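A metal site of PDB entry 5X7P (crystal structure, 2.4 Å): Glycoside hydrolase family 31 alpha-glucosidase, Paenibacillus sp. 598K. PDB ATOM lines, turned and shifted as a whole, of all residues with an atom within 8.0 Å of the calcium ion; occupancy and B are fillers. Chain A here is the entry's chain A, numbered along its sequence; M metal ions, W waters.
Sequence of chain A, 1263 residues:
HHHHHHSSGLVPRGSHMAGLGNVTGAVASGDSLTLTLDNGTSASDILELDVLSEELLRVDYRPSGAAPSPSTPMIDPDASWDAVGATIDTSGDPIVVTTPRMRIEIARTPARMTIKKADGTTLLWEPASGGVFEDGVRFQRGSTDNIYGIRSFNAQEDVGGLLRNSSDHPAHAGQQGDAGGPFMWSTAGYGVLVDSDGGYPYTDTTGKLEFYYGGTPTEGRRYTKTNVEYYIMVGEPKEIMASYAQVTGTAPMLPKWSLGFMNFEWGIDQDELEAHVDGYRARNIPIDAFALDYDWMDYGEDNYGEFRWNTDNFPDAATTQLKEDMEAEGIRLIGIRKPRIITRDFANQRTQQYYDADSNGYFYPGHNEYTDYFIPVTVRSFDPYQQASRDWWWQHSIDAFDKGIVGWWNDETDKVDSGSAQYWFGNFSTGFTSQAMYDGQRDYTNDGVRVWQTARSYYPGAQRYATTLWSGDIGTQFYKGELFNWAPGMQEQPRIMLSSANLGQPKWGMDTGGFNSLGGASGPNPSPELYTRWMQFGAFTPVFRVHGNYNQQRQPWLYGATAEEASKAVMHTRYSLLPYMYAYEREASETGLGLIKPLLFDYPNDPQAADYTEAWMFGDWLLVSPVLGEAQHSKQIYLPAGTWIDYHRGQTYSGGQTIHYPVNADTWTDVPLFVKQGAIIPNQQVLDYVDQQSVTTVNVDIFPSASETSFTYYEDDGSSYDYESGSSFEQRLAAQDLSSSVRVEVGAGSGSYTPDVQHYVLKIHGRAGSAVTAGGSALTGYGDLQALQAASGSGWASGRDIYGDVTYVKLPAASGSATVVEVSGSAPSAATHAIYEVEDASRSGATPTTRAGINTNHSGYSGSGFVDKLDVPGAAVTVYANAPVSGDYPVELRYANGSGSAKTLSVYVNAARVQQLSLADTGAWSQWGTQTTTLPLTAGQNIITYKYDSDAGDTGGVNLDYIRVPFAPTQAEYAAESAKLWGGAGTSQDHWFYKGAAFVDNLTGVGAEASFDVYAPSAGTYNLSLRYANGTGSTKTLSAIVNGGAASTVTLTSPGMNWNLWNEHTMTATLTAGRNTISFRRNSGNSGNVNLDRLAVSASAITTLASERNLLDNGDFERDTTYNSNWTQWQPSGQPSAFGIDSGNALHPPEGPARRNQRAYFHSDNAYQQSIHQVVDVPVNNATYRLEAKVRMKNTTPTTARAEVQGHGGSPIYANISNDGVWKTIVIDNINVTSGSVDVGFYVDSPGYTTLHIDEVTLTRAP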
ATOM      1  N   HIS A 633       9.175   6.457 -25.847  1.00  0.00           N
ATOM      2  CA  HIS A 633       7.827   5.944 -26.124  1.00  0.00           C
ATOM      3  C   HIS A 633       6.680   6.833 -25.583  1.00  0.00           C
ATOM      4  O   HIS A 633       5.545   6.705 -26.035  1.00  0.00           O
ATOM      5  CB  HIS A 633       7.728   4.553 -25.552  1.00  0.00           C
ATOM      6  CG  HIS A 633       8.770   3.623 -26.064  1.00  0.00           C
ATOM      7  ND1 HIS A 633       8.652   2.972 -27.270  1.00  0.00           N
ATOM      8  CD2 HIS A 633       9.927   3.201 -25.519  1.00  0.00           C
ATOM      9  CE1 HIS A 633       9.703   2.194 -27.448  1.00  0.00           C
ATOM     10  NE2 HIS A 633      10.482   2.294 -26.397  1.00  0.00           N
ATOM     11  N   GLU A 973      -5.543   0.451 -32.062  1.00  0.00           N
ATOM     12  CA  GLU A 973      -4.458  -0.197 -31.358  1.00  0.00           C
ATOM     13  C   GLU A 973      -3.743   0.804 -30.455  1.00  0.00           C
ATOM     14  O   GLU A 973      -3.658   2.003 -30.775  1.00  0.00           O
ATOM     15  CB  GLU A 973      -3.477  -0.866 -32.340  1.00  0.00           C
ATOM     16  CG  GLU A 973      -2.524   0.080 -33.068  1.00  0.00           C
ATOM     17  CD  GLU A 973      -1.644  -0.633 -34.101  1.00  0.00           C
ATOM     18  OE1 GLU A 973      -2.136  -0.862 -35.210  1.00  0.00           O
ATOM     19  OE2 GLU A 973      -0.459  -0.970 -33.817  1.00  0.00           O
ATOM     20  N   TYR A 974      -3.227   0.310 -29.341  1.00  0.00           N
ATOM     21  CA  TYR A 974      -2.465   1.129 -28.397  1.00  0.00           C
ATOM     22  C   TYR A 974      -1.229   0.340 -28.018  1.00  0.00           C
ATOM     23  O   TYR A 974      -1.343  -0.825 -27.669  1.00  0.00           O
ATOM     24  CB  TYR A 974      -3.316   1.509 -27.153  1.00  0.00           C
ATOM     25  CG  TYR A 974      -4.592   2.239 -27.503  1.00  0.00           C
ATOM     26  CD1 TYR A 974      -5.765   1.544 -27.835  1.00  0.00           C
ATOM     27  CD2 TYR A 974      -4.633   3.607 -27.518  1.00  0.00           C
ATOM     28  CE1 TYR A 974      -6.927   2.212 -28.167  1.00  0.00           C
ATOM     29  CE2 TYR A 974      -5.795   4.270 -27.841  1.00  0.00           C
ATOM     30  CZ  TYR A 974      -6.922   3.558 -28.185  1.00  0.00           C
ATOM     31  OH  TYR A 974      -8.089   4.248 -28.494  1.00  0.00           O
ATOM     32  N   ALA A 975      -0.058   0.971 -28.121  1.00  0.00           N
ATOM     33  CA  ALA A 975       1.201   0.288 -27.825  1.00  0.00           C
ATOM     34  C   ALA A 975       1.413   0.240 -26.314  1.00  0.00           C
ATOM     35  O   ALA A 975       1.251   1.270 -25.619  1.00  0.00           O
ATOM     36  CB  ALA A 975       2.363   1.009 -28.487  1.00  0.00           C
ATOM     37  N   ALA A 976       1.801  -0.921 -25.820  1.00  0.00           N
ATOM     38  CA  ALA A 976       2.067  -1.113 -24.362  1.00  0.00           C
ATOM     39  C   ALA A 976       3.271  -0.274 -23.869  1.00  0.00           C
ATOM     40  O   ALA A 976       3.193   0.430 -22.838  1.00  0.00           O
ATOM     41  CB  ALA A 976       2.301  -2.586 -24.096  1.00  0.00           C
ATOM     42  N   GLU A 977       4.341  -0.319 -24.654  1.00  0.00           N
ATOM     43  CA  GLU A 977       5.532   0.507 -24.435  1.00  0.00           C
ATOM     44  C   GLU A 977       5.256   2.026 -24.318  1.00  0.00           C
ATOM     45  O   GLU A 977       6.040   2.722 -23.639  1.00  0.00           O
ATOM     46  CB  GLU A 977       6.597   0.274 -25.505  1.00  0.00           C
ATOM     47  CG  GLU A 977       6.119   0.580 -26.928  1.00  0.00           C
ATOM     48  CD  GLU A 977       5.646  -0.676 -27.670  1.00  0.00           C
ATOM     49  OE1 GLU A 977       5.029  -1.543 -27.020  1.00  0.00           O
ATOM     50  OE2 GLU A 977       5.872  -0.780 -28.899  1.00  0.00           O
ATOM     51  N   SER A 978       4.174   2.501 -24.952  1.00  0.00           N
ATOM     52  CA  SER A 978       3.736   3.920 -24.854  1.00  0.00           C
ATOM     53  C   SER A 978       2.674   4.186 -23.779  1.00  0.00           C
ATOM     54  O   SER A 978       2.239   5.327 -23.563  1.00  0.00           O
ATOM     55  CB  SER A 978       3.252   4.439 -26.248  1.00  0.00           C
ATOM     56  OG  SER A 978       4.298   4.413 -27.235  1.00  0.00           O
ATOM     57  N   SER A 988      11.324  -2.993 -23.116  1.00  0.00           N
ATOM     58  CA  SER A 988      12.440  -3.857 -23.408  1.00  0.00           C
ATOM     59  C   SER A 988      12.369  -4.328 -24.851  1.00  0.00           C
ATOM     60  O   SER A 988      11.284  -4.413 -25.453  1.00  0.00           O
ATOM     61  CB  SER A 988      12.380  -5.053 -22.460  1.00  0.00           C
ATOM     62  OG  SER A 988      13.459  -5.948 -22.687  1.00  0.00           O
ATOM     63  N   PHE A 993       9.840 -10.933 -31.683  1.00  0.00           N
ATOM     64  CA  PHE A 993       8.483 -10.911 -32.240  1.00  0.00           C
ATOM     65  C   PHE A 993       7.454 -10.043 -31.536  1.00  0.00           C
ATOM     66  O   PHE A 993       6.256 -10.244 -31.675  1.00  0.00           O
ATOM     67  CB  PHE A 993       7.916 -12.344 -32.460  1.00  0.00           C
ATOM     68  CG  PHE A 993       8.727 -13.186 -33.408  1.00  0.00           C
ATOM     69  CD1 PHE A 993       8.590 -13.049 -34.767  1.00  0.00           C
ATOM     70  CD2 PHE A 993       9.654 -14.134 -32.914  1.00  0.00           C
ATOM     71  CE1 PHE A 993       9.335 -13.842 -35.642  1.00  0.00           C
ATOM     72  CE2 PHE A 993      10.414 -14.905 -33.779  1.00  0.00           C
ATOM     73  CZ  PHE A 993      10.267 -14.770 -35.138  1.00  0.00           C
ATOM     74  N   TYR A 994       7.916  -9.069 -30.768  1.00  0.00           N
ATOM     75  CA  TYR A 994       7.074  -7.931 -30.408  1.00  0.00           C
ATOM     76  C   TYR A 994       6.705  -7.048 -31.626  1.00  0.00           C
ATOM     77  O   TYR A 994       7.460  -6.964 -32.610  1.00  0.00           O
ATOM     78  CB  TYR A 994       7.767  -7.063 -29.347  1.00  0.00           C
ATOM     79  CG  TYR A 994       9.104  -6.514 -29.724  1.00  0.00           C
ATOM     80  CD1 TYR A 994       9.215  -5.327 -30.455  1.00  0.00           C
ATOM     81  CD2 TYR A 994      10.273  -7.171 -29.365  1.00  0.00           C
ATOM     82  CE1 TYR A 994      10.444  -4.802 -30.816  1.00  0.00           C
ATOM     83  CE2 TYR A 994      11.513  -6.653 -29.730  1.00  0.00           C
ATOM     84  CZ  TYR A 994      11.590  -5.450 -30.463  1.00  0.00           C
ATOM     85  OH  TYR A 994      12.830  -4.928 -30.836  1.00  0.00           O
ATOM     86  N   LYS A 995       5.566  -6.367 -31.504  1.00  0.00           N
ATOM     87  CA  LYS A 995       5.171  -5.380 -32.488  1.00  0.00           C
ATOM     88  C   LYS A 995       5.685  -4.033 -32.084  1.00  0.00           C
ATOM     89  O   LYS A 995       6.122  -3.839 -30.956  1.00  0.00           O
ATOM     90  CB  LYS A 995       3.654  -5.381 -32.655  1.00  0.00           C
ATOM     91  CG  LYS A 995       3.084  -6.791 -32.920  1.00  0.00           C
ATOM     92  CD  LYS A 995       3.736  -7.443 -34.134  1.00  0.00           C
ATOM     93  CE  LYS A 995       3.096  -8.800 -34.447  1.00  0.00           C
ATOM     94  NZ  LYS A 995       3.217  -9.169 -35.883  1.00  0.00           N
ATOM     95  N   GLY A 996       5.685  -3.089 -32.999  1.00  0.00           N
ATOM     96  CA  GLY A 996       6.179  -1.764 -32.694  1.00  0.00           C
ATOM     97  C   GLY A 996       7.647  -1.779 -32.320  1.00  0.00           C
ATOM     98  O   GLY A 996       8.422  -2.699 -32.689  1.00  0.00           O
ATOM     99  N   ALA A 997       8.058  -0.743 -31.607  1.00  0.00           N
ATOM    100  CA  ALA A 997       9.487  -0.561 -31.299  1.00  0.00           C
ATOM    101  C   ALA A 997       9.915  -1.220 -29.995  1.00  0.00           C
ATOM    102  O   ALA A 997      11.102  -1.242 -29.698  1.00  0.00           O
ATOM    103  CB  ALA A 997       9.819   0.916 -31.257  1.00  0.00           C
ATOM    104  N   ALA A 998       8.953  -1.715 -29.207  1.00  0.00           N
ATOM    105  CA  ALA A 998       9.256  -2.488 -27.987  1.00  0.00           C
ATOM    106  C   ALA A 998       8.043  -3.280 -27.414  1.00  0.00           C
ATOM    107  O   ALA A 998       6.973  -3.416 -28.087  1.00  0.00           O
ATOM    108  CB  ALA A 998       9.874  -1.564 -26.893  1.00  0.00           C
ATOM    109  N   PHE A 999       8.251  -3.800 -26.196  1.00  0.00           N
ATOM    110  CA  PHE A 999       7.179  -4.364 -25.370  1.00  0.00           C
ATOM    111  C   PHE A 999       7.367  -3.969 -23.881  1.00  0.00           C
ATOM    112  O   PHE A 999       8.342  -3.313 -23.546  1.00  0.00           O
ATOM    113  CB  PHE A 999       7.102  -5.882 -25.591  1.00  0.00           C
ATOM    114  CG  PHE A 999       8.334  -6.607 -25.203  1.00  0.00           C
ATOM    115  CD1 PHE A 999       8.538  -7.036 -23.894  1.00  0.00           C
ATOM    116  CD2 PHE A 999       9.289  -6.887 -26.145  1.00  0.00           C
ATOM    117  CE1 PHE A 999       9.711  -7.674 -23.526  1.00  0.00           C
ATOM    118  CE2 PHE A 999      10.465  -7.524 -25.821  1.00  0.00           C
ATOM    119  CZ  PHE A 999      10.674  -7.929 -24.512  1.00  0.00           C
ATOM    120  N   VAL A1000       6.426  -4.349 -23.014  1.00  0.00           N
ATOM    121  CA  VAL A1000       6.498  -4.065 -21.586  1.00  0.00           C
ATOM    122  C   VAL A1000       6.775  -5.347 -20.823  1.00  0.00           C
ATOM    123  O   VAL A1000       6.021  -6.322 -20.948  1.00  0.00           O
ATOM    124  CB  VAL A1000       5.186  -3.501 -21.032  1.00  0.00           C
ATOM    125  CG1 VAL A1000       5.226  -3.522 -19.498  1.00  0.00           C
ATOM    126  CG2 VAL A1000       4.908  -2.087 -21.561  1.00  0.00           C
ATOM    127  N   ARG A1027      -2.168  -8.417 -26.458  1.00  0.00           N
ATOM    128  CA  ARG A1027      -1.075  -9.263 -26.929  1.00  0.00           C
ATOM    129  C   ARG A1027      -0.013  -9.340 -25.847  1.00  0.00           C
ATOM    130  O   ARG A1027       0.567  -8.299 -25.444  1.00  0.00           O
ATOM    131  CB  ARG A1027      -0.486  -8.711 -28.229  1.00  0.00           C
ATOM    132  CG  ARG A1027       0.496  -9.645 -28.941  1.00  0.00           C
ATOM    133  CD  ARG A1027       0.884  -9.091 -30.319  1.00  0.00           C
ATOM    134  NE  ARG A1027       1.493 -10.106 -31.187  1.00  0.00           N
ATOM    135  CZ  ARG A1027       2.798 -10.371 -31.322  1.00  0.00           C
ATOM    136  NH1 ARG A1027       3.710  -9.711 -30.601  1.00  0.00           N
ATOM    137  NH2 ARG A1027       3.199 -11.330 -32.173  1.00  0.00           N
ATOM    138  N   TRP A1062       3.873 -15.057 -28.670  1.00  0.00           N
ATOM    139  CA  TRP A1062       2.848 -14.072 -28.300  1.00  0.00           C
ATOM    140  C   TRP A1062       1.439 -14.630 -28.608  1.00  0.00           C
ATOM    141  O   TRP A1062       1.248 -15.270 -29.648  1.00  0.00           O
ATOM    142  CB  TRP A1062       3.140 -12.762 -29.069  1.00  0.00           C
ATOM    143  CG  TRP A1062       4.552 -12.181 -28.738  1.00  0.00           C
ATOM    144  CD1 TRP A1062       5.732 -12.499 -29.342  1.00  0.00           C
ATOM    145  CD2 TRP A1062       4.879 -11.219 -27.722  1.00  0.00           C
ATOM    146  NE1 TRP A1062       6.772 -11.821 -28.775  1.00  0.00           N
ATOM    147  CE2 TRP A1062       6.296 -11.024 -27.778  1.00  0.00           C
ATOM    148  CE3 TRP A1062       4.132 -10.481 -26.785  1.00  0.00           C
ATOM    149  CZ2 TRP A1062       6.965 -10.129 -26.937  1.00  0.00           C
ATOM    150  CZ3 TRP A1062       4.816  -9.615 -25.904  1.00  0.00           C
ATOM    151  CH2 TRP A1062       6.210  -9.448 -26.005  1.00  0.00           C
ATOM    152  N   LEU A1092       3.640  -7.635 -21.999  1.00  0.00           N
ATOM    153  CA  LEU A1092       2.524  -7.076 -22.724  1.00  0.00           C
ATOM    154  C   LEU A1092       3.079  -6.257 -23.888  1.00  0.00           C
ATOM    155  O   LEU A1092       4.155  -5.671 -23.795  1.00  0.00           O
ATOM    156  CB  LEU A1092       1.713  -6.178 -21.815  1.00  0.00           C
ATOM    157  CG  LEU A1092       1.238  -6.787 -20.505  1.00  0.00           C
ATOM    158  CD1 LEU A1092       0.424  -5.730 -19.796  1.00  0.00           C
ATOM    159  CD2 LEU A1092       0.431  -8.075 -20.673  1.00  0.00           C
ATOM    160  N   ASP A1093       2.329  -6.204 -24.976  1.00  0.00           N
ATOM    161  CA  ASP A1093       2.857  -5.620 -26.211  1.00  0.00           C
ATOM    162  C   ASP A1093       1.932  -4.557 -26.816  1.00  0.00           C
ATOM    163  O   ASP A1093       2.399  -3.466 -27.121  1.00  0.00           O
ATOM    164  CB  ASP A1093       3.178  -6.748 -27.177  1.00  0.00           C
ATOM    165  CG  ASP A1093       3.938  -6.292 -28.410  1.00  0.00           C
ATOM    166  OD1 ASP A1093       4.598  -5.233 -28.383  1.00  0.00           O
ATOM    167  OD2 ASP A1093       3.880  -7.031 -29.418  1.00  0.00           O
ATOM    168  N   ARG A1094       0.635  -4.881 -26.922  1.00  0.00           N
ATOM    169  CA  ARG A1094      -0.376  -4.020 -27.578  1.00  0.00           C
ATOM    170  C   ARG A1094      -1.809  -4.429 -27.137  1.00  0.00           C
ATOM    171  O   ARG A1094      -2.114  -5.617 -26.946  1.00  0.00           O
ATOM    172  CB  ARG A1094      -0.216  -4.115 -29.125  1.00  0.00           C
ATOM    173  CG  ARG A1094      -1.259  -3.389 -29.960  1.00  0.00           C
ATOM    174  CD  ARG A1094      -2.493  -4.238 -30.244  1.00  0.00           C
ATOM    175  NE  ARG A1094      -2.179  -5.432 -31.018  1.00  0.00           N
ATOM    176  CZ  ARG A1094      -2.609  -6.680 -30.749  1.00  0.00           C
ATOM    177  NH1 ARG A1094      -3.402  -6.978 -29.725  1.00  0.00           N
ATOM    178  NH2 ARG A1094      -2.238  -7.659 -31.553  1.00  0.00           N
ATOM    179  N   LEU A1095      -2.643  -3.420 -26.967  1.00  0.00           N
ATOM    180  CA  LEU A1095      -4.079  -3.564 -26.751  1.00  0.00           C
ATOM    181  C   LEU A1095      -4.799  -3.087 -27.998  1.00  0.00           C
ATOM    182  O   LEU A1095      -4.636  -1.930 -28.444  1.00  0.00           O
ATOM    183  CB  LEU A1095      -4.522  -2.679 -25.599  1.00  0.00           C
ATOM    184  CG  LEU A1095      -5.982  -2.778 -25.146  1.00  0.00           C
ATOM    185  CD1 LEU A1095      -6.255  -4.138 -24.516  1.00  0.00           C
ATOM    186  CD2 LEU A1095      -6.299  -1.672 -24.158  1.00  0.00           C
ATOM    187  N   GLU A1108       0.547  -5.005 -38.220  1.00  0.00           N
ATOM    188  CA  GLU A1108       1.131  -6.202 -37.609  1.00  0.00           C
ATOM    189  C   GLU A1108       1.255  -7.359 -38.589  1.00  0.00           C
ATOM    190  O   GLU A1108       1.402  -8.480 -38.153  1.00  0.00           O
ATOM    191  CB  GLU A1108       0.308  -6.612 -36.337  1.00  0.00           C
ATOM    192  CG  GLU A1108       0.319  -5.536 -35.247  1.00  0.00           C
ATOM    193  CD  GLU A1108      -0.394  -5.940 -33.956  1.00  0.00           C
ATOM    194  OE1 GLU A1108      -0.934  -7.056 -33.884  1.00  0.00           O
ATOM    195  OE2 GLU A1108      -0.439  -5.141 -32.981  1.00  0.00           O
HETATM  196 CA    CA M   1       4.742  -3.164 -28.930  1.00  0.00          CA
HETATM  197  O   HOH W   1       2.657  -2.338 -30.389  1.00  0.00           O
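The side-chain amino group (NZ) of Lys 995 lies within hydrogen-bond range of the backbone carbonyl oxygen (O) of Glu 1108. The side-chain carboxylate (OE2) of Glu 977 lies close to the backbone NH (N) of Ala 997 (3.5 Å). The guanidinium group of Arg 1027 lies within salt-bridge range of the side-chain carboxylate of Asp 1093, at 2.9 Å. The backbone carbonyl oxygen of Asp 1093 is in hydrogen-bond range of the backbone NH of Ala 976, at 2.9 Å.
The calcium ion is bound by the side-chain carboxylate (OD1) of Asp 1093 (2.1 Å), the backbone carbonyl oxygen (O) of Ala 998 (2.4 Å), the side-chain carboxylate (OE1) of Glu 977 (2.5 Å), the backbone carbonyl oxygen (O) of Lys 995 (2.5 Å), the side-chain carboxylate (OE2) of Glu 977 (2.6 Å) and water W1 (2.7 Å). The calcium ion has six donor atoms within binding distance. Slightly farther from the calcium ion lies O of Asp 1093 (3.0 Å).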
